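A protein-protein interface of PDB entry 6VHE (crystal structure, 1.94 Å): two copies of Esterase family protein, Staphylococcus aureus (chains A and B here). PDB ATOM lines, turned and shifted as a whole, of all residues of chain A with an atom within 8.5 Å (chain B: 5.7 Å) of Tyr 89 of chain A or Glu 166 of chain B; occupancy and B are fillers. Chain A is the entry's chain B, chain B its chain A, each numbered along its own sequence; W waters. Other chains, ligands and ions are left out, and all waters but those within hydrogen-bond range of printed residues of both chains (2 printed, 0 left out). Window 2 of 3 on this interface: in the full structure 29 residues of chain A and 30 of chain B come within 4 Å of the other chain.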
ATOM      1  N   SER A  82      33.469 -30.598  23.097  1.00  0.00           N
ATOM      2  CA  SER A  82      33.824 -30.032  21.800  1.00  0.00           C
ATOM      3  C   SER A  82      34.456 -31.027  20.839  1.00  0.00           C
ATOM      4  O   SER A  82      34.655 -30.675  19.675  1.00  0.00           O
ATOM      5  CB  SER A  82      34.800 -28.877  21.989  1.00  0.00           C
ATOM      6  OG  SER A  82      36.072 -29.378  22.402  1.00  0.00           O
ATOM      7  N   ALA A  85      37.478 -29.801  18.504  1.00  0.00           N
ATOM      8  CA  ALA A  85      37.288 -29.105  17.241  1.00  0.00           C
ATOM      9  C   ALA A  85      37.121 -27.610  17.474  1.00  0.00           C
ATOM     10  O   ALA A  85      36.676 -27.176  18.541  1.00  0.00           O
ATOM     11  CB  ALA A  85      36.058 -29.633  16.503  1.00  0.00           C
ATOM     12  N   ASN A  86      37.477 -26.828  16.462  1.00  0.00           N
ATOM     13  CA  ASN A  86      36.958 -25.467  16.340  1.00  0.00           C
ATOM     14  C   ASN A  86      35.482 -25.588  15.983  1.00  0.00           C
ATOM     15  O   ASN A  86      35.131 -25.861  14.838  1.00  0.00           O
ATOM     16  CB  ASN A  86      37.729 -24.681  15.283  1.00  0.00           C
ATOM     17  CG  ASN A  86      39.158 -24.393  15.707  1.00  0.00           C
ATOM     18  OD1 ASN A  86      39.436 -24.257  16.895  1.00  0.00           O
ATOM     19  ND2 ASN A  86      40.070 -24.295  14.740  1.00  0.00           N
ATOM     20  N   MET A  87      34.605 -25.398  16.967  1.00  0.00           N
ATOM     21  CA  MET A  87      33.202 -25.771  16.805  1.00  0.00           C
ATOM     22  C   MET A  87      32.457 -24.839  15.855  1.00  0.00           C
ATOM     23  O   MET A  87      32.705 -23.625  15.811  1.00  0.00           O
ATOM     24  CB  MET A  87      32.500 -25.773  18.158  1.00  0.00           C
ATOM     25  CG  MET A  87      33.160 -26.691  19.191  1.00  0.00           C
ATOM     26  SD  MET A  87      32.579 -26.370  20.865  1.00  0.00           S
ATOM     27  CE  MET A  87      30.872 -26.942  20.796  1.00  0.00           C
ATOM     28  N   ALA A  88      31.516 -25.428  15.104  1.00  0.00           N
ATOM     29  CA  ALA A  88      30.641 -24.642  14.241  1.00  0.00           C
ATOM     30  C   ALA A  88      29.851 -23.622  15.050  1.00  0.00           C
ATOM     31  O   ALA A  88      29.739 -22.458  14.658  1.00  0.00           O
ATOM     32  CB  ALA A  88      29.690 -25.570  13.468  1.00  0.00           C
ATOM     33  N   TYR A  89      29.284 -24.050  16.183  1.00  0.00           N
ATOM     34  CA  TYR A  89      28.531 -23.183  17.091  1.00  0.00           C
ATOM     35  C   TYR A  89      29.074 -23.459  18.493  1.00  0.00           C
ATOM     36  O   TYR A  89      28.570 -24.332  19.203  1.00  0.00           O
ATOM     37  CB  TYR A  89      27.027 -23.442  17.012  1.00  0.00           C
ATOM     38  CG  TYR A  89      26.463 -23.452  15.599  1.00  0.00           C
ATOM     39  CD1 TYR A  89      25.911 -24.611  15.065  1.00  0.00           C
ATOM     40  CD2 TYR A  89      26.473 -22.310  14.818  1.00  0.00           C
ATOM     41  CE1 TYR A  89      25.391 -24.632  13.784  1.00  0.00           C
ATOM     42  CE2 TYR A  89      25.949 -22.318  13.532  1.00  0.00           C
ATOM     43  CZ  TYR A  89      25.413 -23.484  13.023  1.00  0.00           C
ATOM     44  OH  TYR A  89      24.893 -23.510  11.753  1.00  0.00           O
ATOM     45  N   GLY A  90      30.111 -22.736  18.881  1.00  0.00           N
ATOM     46  CA  GLY A  90      30.739 -22.985  20.167  1.00  0.00           C
ATOM     47  C   GLY A  90      32.077 -22.290  20.280  1.00  0.00           C
ATOM     48  O   GLY A  90      32.196 -21.126  19.884  1.00  0.00           O
ATOM     49  N   HIS A  91      33.090 -22.981  20.804  1.00  0.00           N
ATOM     50  CA  HIS A  91      34.399 -22.394  21.030  1.00  0.00           C
ATOM     51  C   HIS A  91      35.420 -22.956  20.062  1.00  0.00           C
ATOM     52  O   HIS A  91      35.266 -24.055  19.520  1.00  0.00           O
ATOM     53  CB  HIS A  91      34.906 -22.649  22.457  1.00  0.00           C
ATOM     54  CG  HIS A  91      34.157 -21.888  23.499  1.00  0.00           C
ATOM     55  ND1 HIS A  91      34.366 -20.545  23.729  1.00  0.00           N
ATOM     56  CD2 HIS A  91      33.186 -22.274  24.358  1.00  0.00           C
ATOM     57  CE1 HIS A  91      33.564 -20.139  24.695  1.00  0.00           C
ATOM     58  NE2 HIS A  91      32.841 -21.170  25.098  1.00  0.00           N
ATOM     59  N   SER A  92      36.513 -22.207  19.928  1.00  0.00           N
ATOM     60  CA  SER A  92      37.627 -22.564  19.046  1.00  0.00           C
ATOM     61  C   SER A  92      38.582 -23.505  19.791  1.00  0.00           C
ATOM     62  O   SER A  92      39.715 -23.161  20.140  1.00  0.00           O
ATOM     63  CB  SER A  92      38.339 -21.294  18.596  1.00  0.00           C
ATOM     64  OG  SER A  92      37.487 -20.477  17.814  1.00  0.00           O
ATOM     65  N   TYR A  93      38.105 -24.733  20.045  1.00  0.00           N
ATOM     66  CA  TYR A  93      38.820 -25.594  20.980  1.00  0.00           C
ATOM     67  C   TYR A  93      40.008 -26.315  20.353  1.00  0.00           C
ATOM     68  O   TYR A  93      40.932 -26.697  21.081  1.00  0.00           O
ATOM     69  CB  TYR A  93      37.865 -26.611  21.603  1.00  0.00           C
ATOM     70  CG  TYR A  93      37.248 -26.150  22.893  1.00  0.00           C
ATOM     71  CD1 TYR A  93      38.042 -25.843  24.009  1.00  0.00           C
ATOM     72  CD2 TYR A  93      35.868 -26.013  23.012  1.00  0.00           C
ATOM     73  CE1 TYR A  93      37.466 -25.418  25.195  1.00  0.00           C
ATOM     74  CE2 TYR A  93      35.282 -25.619  24.216  1.00  0.00           C
ATOM     75  CZ  TYR A  93      36.091 -25.317  25.293  1.00  0.00           C
ATOM     76  OH  TYR A  93      35.515 -24.915  26.468  1.00  0.00           O
ATOM     77  N   SER A 164      25.900 -32.248  21.940  1.00  0.00           N
ATOM     78  CA  SER A 164      25.347 -31.633  20.728  1.00  0.00           C
ATOM     79  C   SER A 164      26.304 -31.852  19.562  1.00  0.00           C
ATOM     80  O   SER A 164      27.380 -31.242  19.508  1.00  0.00           O
ATOM     81  CB  SER A 164      25.085 -30.137  20.913  1.00  0.00           C
ATOM     82  OG  SER A 164      24.692 -29.527  19.681  1.00  0.00           O
ATOM     83  N   LYS A 165      25.894 -32.705  18.619  1.00  0.00           N
ATOM     84  CA  LYS A 165      26.663 -32.917  17.391  1.00  0.00           C
ATOM     85  C   LYS A 165      26.725 -31.649  16.538  1.00  0.00           C
ATOM     86  O   LYS A 165      27.787 -31.291  16.011  1.00  0.00           O
ATOM     87  CB  LYS A 165      26.041 -34.064  16.585  1.00  0.00           C
ATOM     88  CG  LYS A 165      26.627 -34.232  15.186  1.00  0.00           C
ATOM     89  CD  LYS A 165      25.560 -34.216  14.100  1.00  0.00           C
ATOM     90  CE  LYS A 165      24.783 -35.519  14.056  1.00  0.00           C
ATOM     91  NZ  LYS A 165      24.310 -35.820  12.674  1.00  0.00           N
ATOM     92  N   GLU A 166      25.585 -30.975  16.362  1.00  0.00           N
ATOM     93  CA  GLU A 166      25.559 -29.767  15.544  1.00  0.00           C
ATOM     94  C   GLU A 166      26.466 -28.677  16.108  1.00  0.00           C
ATOM     95  O   GLU A 166      27.000 -27.864  15.342  1.00  0.00           O
ATOM     96  CB  GLU A 166      24.135 -29.235  15.416  1.00  0.00           C
ATOM     97  CG  GLU A 166      23.188 -30.115  14.609  1.00  0.00           C
ATOM     98  CD  GLU A 166      22.506 -31.183  15.457  1.00  0.00           C
ATOM     99  OE1 GLU A 166      22.859 -31.331  16.654  1.00  0.00           O
ATOM    100  OE2 GLU A 166      21.609 -31.869  14.921  1.00  0.00           O
ATOM    101  N   ALA A 167      26.623 -28.616  17.436  1.00  0.00           N
ATOM    102  CA  ALA A 167      27.551 -27.651  18.011  1.00  0.00           C
ATOM    103  C   ALA A 167      28.932 -27.821  17.399  1.00  0.00           C
ATOM    104  O   ALA A 167      29.597 -26.838  17.053  1.00  0.00           O
ATOM    105  CB  ALA A 167      27.611 -27.806  19.531  1.00  0.00           C
ATOM    106  N   ILE A 168      29.350 -29.067  17.202  1.00  0.00           N
ATOM    107  CA  ILE A 168      30.673 -29.330  16.658  1.00  0.00           C
ATOM    108  C   ILE A 168      30.701 -29.095  15.158  1.00  0.00           C
ATOM    109  O   ILE A 168      31.515 -28.307  14.664  1.00  0.00           O
ATOM    110  CB  ILE A 168      31.123 -30.757  17.010  1.00  0.00           C
ATOM    111  CG1 ILE A 168      31.137 -30.936  18.533  1.00  0.00           C
ATOM    112  CG2 ILE A 168      32.515 -31.012  16.461  1.00  0.00           C
ATOM    113  CD1 ILE A 168      31.355 -32.368  18.971  1.00  0.00           C
ATOM    114  N   ILE A 169      29.829 -29.772  14.405  1.00  0.00           N
ATOM    115  CA  ILE A 169      29.977 -29.853  12.954  1.00  0.00           C
ATOM    116  C   ILE A 169      28.917 -29.070  12.191  1.00  0.00           C
ATOM    117  O   ILE A 169      28.927 -29.096  10.952  1.00  0.00           O
ATOM    118  CB  ILE A 169      30.004 -31.318  12.480  1.00  0.00           C
ATOM    119  CG1 ILE A 169      28.621 -31.958  12.623  1.00  0.00           C
ATOM    120  CG2 ILE A 169      31.041 -32.097  13.269  1.00  0.00           C
ATOM    121  CD1 ILE A 169      28.555 -33.399  12.155  1.00  0.00           C
ATOM    122  N   GLY A 170      28.015 -28.376  12.869  1.00  0.00           N
ATOM    123  CA  GLY A 170      27.049 -27.556  12.150  1.00  0.00           C
ATOM    124  C   GLY A 170      26.098 -28.405  11.325  1.00  0.00           C
ATOM    125  O   GLY A 170      25.497 -29.361  11.828  1.00  0.00           O
ATOM    126  N   ASN A 171      25.978 -28.066  10.035  1.00  0.00           N
ATOM    127  CA  ASN A 171      24.996 -28.651   9.121  1.00  0.00           C
ATOM    128  C   ASN A 171      25.458 -29.947   8.472  1.00  0.00           C
ATOM    129  O   ASN A 171      24.677 -30.555   7.732  1.00  0.00           O
ATOM    130  CB  ASN A 171      24.648 -27.661   8.003  1.00  0.00           C
ATOM    131  CG  ASN A 171      23.743 -26.561   8.466  1.00  0.00           C
ATOM    132  OD1 ASN A 171      23.009 -26.720   9.443  1.00  0.00           O
ATOM    133  ND2 ASN A 171      23.773 -25.430   7.763  1.00  0.00           N
ATOM    134  N   LEU A 172      26.693 -30.369   8.708  1.00  0.00           N
ATOM    135  CA  LEU A 172      27.263 -31.501   7.990  1.00  0.00           C
ATOM    136  C   LEU A 172      26.455 -32.774   8.199  1.00  0.00           C
ATOM    137  O   LEU A 172      26.262 -33.221   9.331  1.00  0.00           O
ATOM    138  CB  LEU A 172      28.698 -31.735   8.452  1.00  0.00           C
ATOM    139  CG  LEU A 172      29.801 -30.906   7.817  1.00  0.00           C
ATOM    140  CD1 LEU A 172      31.147 -31.416   8.335  1.00  0.00           C
ATOM    141  CD2 LEU A 172      29.706 -30.990   6.287  1.00  0.00           C
ATOM    142  N   ALA B  88      20.415 -23.996  22.009  1.00  0.00           N
ATOM    143  CA  ALA B  88      19.975 -24.739  20.834  1.00  0.00           C
ATOM    144  C   ALA B  88      21.032 -25.747  20.399  1.00  0.00           C
ATOM    145  O   ALA B  88      20.707 -26.868  19.998  1.00  0.00           O
ATOM    146  CB  ALA B  88      19.654 -23.768  19.695  1.00  0.00           C
ATOM    147  N   TYR B  89      22.309 -25.370  20.478  1.00  0.00           N
ATOM    148  CA  TYR B  89      23.422 -26.256  20.122  1.00  0.00           C
ATOM    149  C   TYR B  89      24.455 -26.098  21.227  1.00  0.00           C
ATOM    150  O   TYR B  89      25.325 -25.231  21.138  1.00  0.00           O
ATOM    151  CB  TYR B  89      24.017 -25.912  18.755  1.00  0.00           C
ATOM    152  CG  TYR B  89      23.004 -25.786  17.637  1.00  0.00           C
ATOM    153  CD1 TYR B  89      22.802 -24.577  16.995  1.00  0.00           C
ATOM    154  CD2 TYR B  89      22.246 -26.877  17.233  1.00  0.00           C
ATOM    155  CE1 TYR B  89      21.872 -24.453  15.968  1.00  0.00           C
ATOM    156  CE2 TYR B  89      21.316 -26.765  16.210  1.00  0.00           C
ATOM    157  CZ  TYR B  89      21.134 -25.550  15.580  1.00  0.00           C
ATOM    158  OH  TYR B  89      20.215 -25.432  14.560  1.00  0.00           O
ATOM    159  N   SER B 164      29.290 -17.341  20.388  1.00  0.00           N
ATOM    160  CA  SER B 164      28.423 -17.878  19.335  1.00  0.00           C
ATOM    161  C   SER B 164      26.958 -17.568  19.661  1.00  0.00           C
ATOM    162  O   SER B 164      26.375 -18.152  20.583  1.00  0.00           O
ATOM    163  CB  SER B 164      28.630 -19.390  19.159  1.00  0.00           C
ATOM    164  OG  SER B 164      27.588 -19.957  18.350  1.00  0.00           O
ATOM    165  N   LYS B 165      26.354 -16.667  18.884  1.00  0.00           N
ATOM    166  CA  LYS B 165      24.926 -16.399  19.027  1.00  0.00           C
ATOM    167  C   LYS B 165      24.108 -17.647  18.716  1.00  0.00           C
ATOM    168  O   LYS B 165      23.219 -18.030  19.488  1.00  0.00           O
ATOM    169  CB  LYS B 165      24.497 -15.253  18.104  1.00  0.00           C
ATOM    170  CG  LYS B 165      22.986 -15.074  18.044  1.00  0.00           C
ATOM    171  CD  LYS B 165      22.559 -13.900  17.160  1.00  0.00           C
ATOM    172  CE  LYS B 165      22.533 -14.265  15.678  1.00  0.00           C
ATOM    173  NZ  LYS B 165      21.533 -13.435  14.939  1.00  0.00           N
ATOM    174  N   GLU B 166      24.435 -18.313  17.608  1.00  0.00           N
ATOM    175  CA  GLU B 166      23.640 -19.439  17.132  1.00  0.00           C
ATOM    176  C   GLU B 166      23.671 -20.599  18.109  1.00  0.00           C
ATOM    177  O   GLU B 166      22.682 -21.321  18.238  1.00  0.00           O
ATOM    178  CB  GLU B 166      24.141 -19.908  15.767  1.00  0.00           C
ATOM    179  CG  GLU B 166      23.799 -18.994  14.607  1.00  0.00           C
ATOM    180  CD  GLU B 166      24.725 -17.798  14.528  1.00  0.00           C
ATOM    181  OE1 GLU B 166      25.687 -17.731  15.331  1.00  0.00           O
ATOM    182  OE2 GLU B 166      24.486 -16.926  13.664  1.00  0.00           O
ATOM    183  N   ALA B 167      24.809 -20.816  18.780  1.00  0.00           N
ATOM    184  CA  ALA B 167      24.858 -21.831  19.830  1.00  0.00           C
ATOM    185  C   ALA B 167      23.708 -21.655  20.810  1.00  0.00           C
ATOM    186  O   ALA B 167      23.073 -22.636  21.217  1.00  0.00           O
ATOM    187  CB  ALA B 167      26.193 -21.773  20.574  1.00  0.00           C
ATOM    188  N   ILE B 168      23.404 -20.406  21.177  1.00  0.00           N
ATOM    189  CA  ILE B 168      22.363 -20.168  22.172  1.00  0.00           C
ATOM    190  C   ILE B 168      20.984 -20.292  21.547  1.00  0.00           C
ATOM    191  O   ILE B 168      20.132 -21.038  22.042  1.00  0.00           O
ATOM    192  CB  ILE B 168      22.547 -18.793  22.837  1.00  0.00           C
ATOM    193  CG1 ILE B 168      23.849 -18.749  23.641  1.00  0.00           C
ATOM    194  CG2 ILE B 168      21.343 -18.468  23.732  1.00  0.00           C
ATOM    195  CD1 ILE B 168      24.307 -17.348  23.990  1.00  0.00           C
ATOM    196  N   ILE B 169      20.745 -19.576  20.446  1.00  0.00           N
ATOM    197  CA  ILE B 169      19.397 -19.380  19.929  1.00  0.00           C
ATOM    198  C   ILE B 169      19.162 -20.055  18.590  1.00  0.00           C
ATOM    199  O   ILE B 169      18.047 -19.945  18.049  1.00  0.00           O
ATOM    200  CB  ILE B 169      19.052 -17.882  19.828  1.00  0.00           C
ATOM    201  CG1 ILE B 169      19.932 -17.205  18.775  1.00  0.00           C
ATOM    202  CG2 ILE B 169      19.168 -17.198  21.198  1.00  0.00           C
ATOM    203  CD1 ILE B 169      19.518 -15.802  18.448  1.00  0.00           C
ATOM    204  N   GLY B 170      20.151 -20.748  18.030  1.00  0.00           N
ATOM    205  CA  GLY B 170      19.894 -21.413  16.760  1.00  0.00           C
ATOM    206  C   GLY B 170      19.745 -20.406  15.641  1.00  0.00           C
ATOM    207  O   GLY B 170      20.495 -19.426  15.543  1.00  0.00           O
ATOM    208  N   ASN B 171      18.763 -20.633  14.781  1.00  0.00           N
ATOM    209  CA  ASN B 171      18.562 -19.754  13.637  1.00  0.00           C
ATOM    210  C   ASN B 171      17.428 -18.756  13.855  1.00  0.00           C
ATOM    211  O   ASN B 171      16.811 -18.294  12.892  1.00  0.00           O
ATOM    212  CB  ASN B 171      18.343 -20.577  12.367  1.00  0.00           C
ATOM    213  CG  ASN B 171      19.641 -21.120  11.820  1.00  0.00           C
ATOM    214  OD1 ASN B 171      20.020 -22.258  12.102  1.00  0.00           O
ATOM    215  ND2 ASN B 171      20.346 -20.297  11.045  1.00  0.00           N
HETATM  216  O   HOH W   1      27.923 -24.781  21.713  1.00  0.00           O
HETATM  217  O   HOH W   2      31.022 -19.296  22.317  1.00  0.00           O
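Tyr 89 of chain B touches Tyr 89 of chain A.
Ser 164 of chain B touches Tyr 89 of chain A (OG to CA, 3.6 Å).
CD2 of Tyr 89 of chain A touches CB of Glu 166 of chain B, at 3.5 Å.
O of Tyr 89 of chain A touches CB of Ala 167 of chain B, at 3.8 Å.
N of Gly 90 of chain A touches CB of Ser 164 of chain B, at 3.7 Å.
Tyr 89 of chain B touches Ser 164 of chain A (CA to OG, 3.5 Å).
Tyr 89 of chain B touches Glu 166 of chain A.
CB of Ala 167 of chain A touches O of Tyr 89 of chain B, at 3.8 Å.
Tyr 89 of chain B touches its own counterpart, Tyr 89 of chain A.
Tyr 89 of chain A touches Ser 164 of chain B, and with the chains exchanged Ser 164 of chain A touches Tyr 89 of chain B.
Tyr 89 of chain A touches Glu 166 of chain B, and with the chains exchanged Glu 166 of chain A touches Tyr 89 of chain B.
Tyr 89 of chain A touches Ala 167 of chain B, and with the chains exchanged Ala 167 of chain A touches Tyr 89 of chain B.
Positions printed for both chains: 88, 89, 164, 165, 166, 167, 168, 169, 170 and 171.
Hydrophobic or aromatic side chains of chain A that line the printed part of chain B: Tyr 89 and Ala 167.
Of the 10 printed residues of chain B, 4 touch a printed residue of chain A.
Among the printed residues, 8 pairs touch across the chains.
Among the printed residues, no Asp or Glu carboxylate lies within 4 Å of a Lys or Arg side-chain nitrogen of the other chain.
N of Ala 167 of chain B lies within hydrogen-bond range of OG of Ser 164 of chain B, at 2.9 Å.
The backbone NH of Tyr 89 of chain A is in hydrogen-bond range of the backbone carbonyl oxygen of Ala 167 of chain A, 2.9 Å away.
N of Ala 88 of chain B is in hydrogen-bond range of O of Ala 167 of chain B.
The backbone NH (N) of Ala 167 of chain A is in hydrogen-bond range of the side-chain hydroxyl (OG) of Ser 164 of chain A (3.1 Å).
The backbone NH (N) of Tyr 89 of chain B sits at hydrogen-bond distance from the backbone carbonyl oxygen (O) of Ala 167 of chain B (2.9 Å).
N of Ala 88 of chain A sits at hydrogen-bond distance from O of Ala 167 of chain A, at 3.1 Å.
Water W1 bridges O of Tyr 89 of chain A (2.6 Å) and O of Tyr 89 of chain B (2.7 Å).
Water W2 lies within hydrogen-bond range of the backbone NH of Ser 164 of chain B (3.2 Å) and the backbone carbonyl oxygen of Gly 90 of chain A (3.3 Å).
Of chain B, only Tyr 89, Ser 164, Glu 166 and Ala 167 come within 4 Å of Tyr 89 of chain A.
Printed residues of chain B within 4 Å of Ser 164 of chain A: Tyr 89 (3.5 Å).
Of the printed residues of chain B, Ala 167 of chain A touches Tyr 89.
Of the printed residues of chain A, Tyr 89 of chain B touches Tyr 89, Ser 164, Glu 166 and Ala 167.
Printed residues of chain A within 4 Å of Glu 166 of chain B: Tyr 89.
Of chain A, only Tyr 89 (3.8 Å) comes within 4 Å of Ala 167 of chain B.
No residue of chain A comes within 4 Å of Gly 170 of chain B.
The nearest residue of chain A that does not touch Glu 166 of chain B is Ala 88 of chain A (6.3 Å).
The nearest printed residue of chain B that does not touch Gly 90 of chain A is Ala 167 of chain B (4.4 Å).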
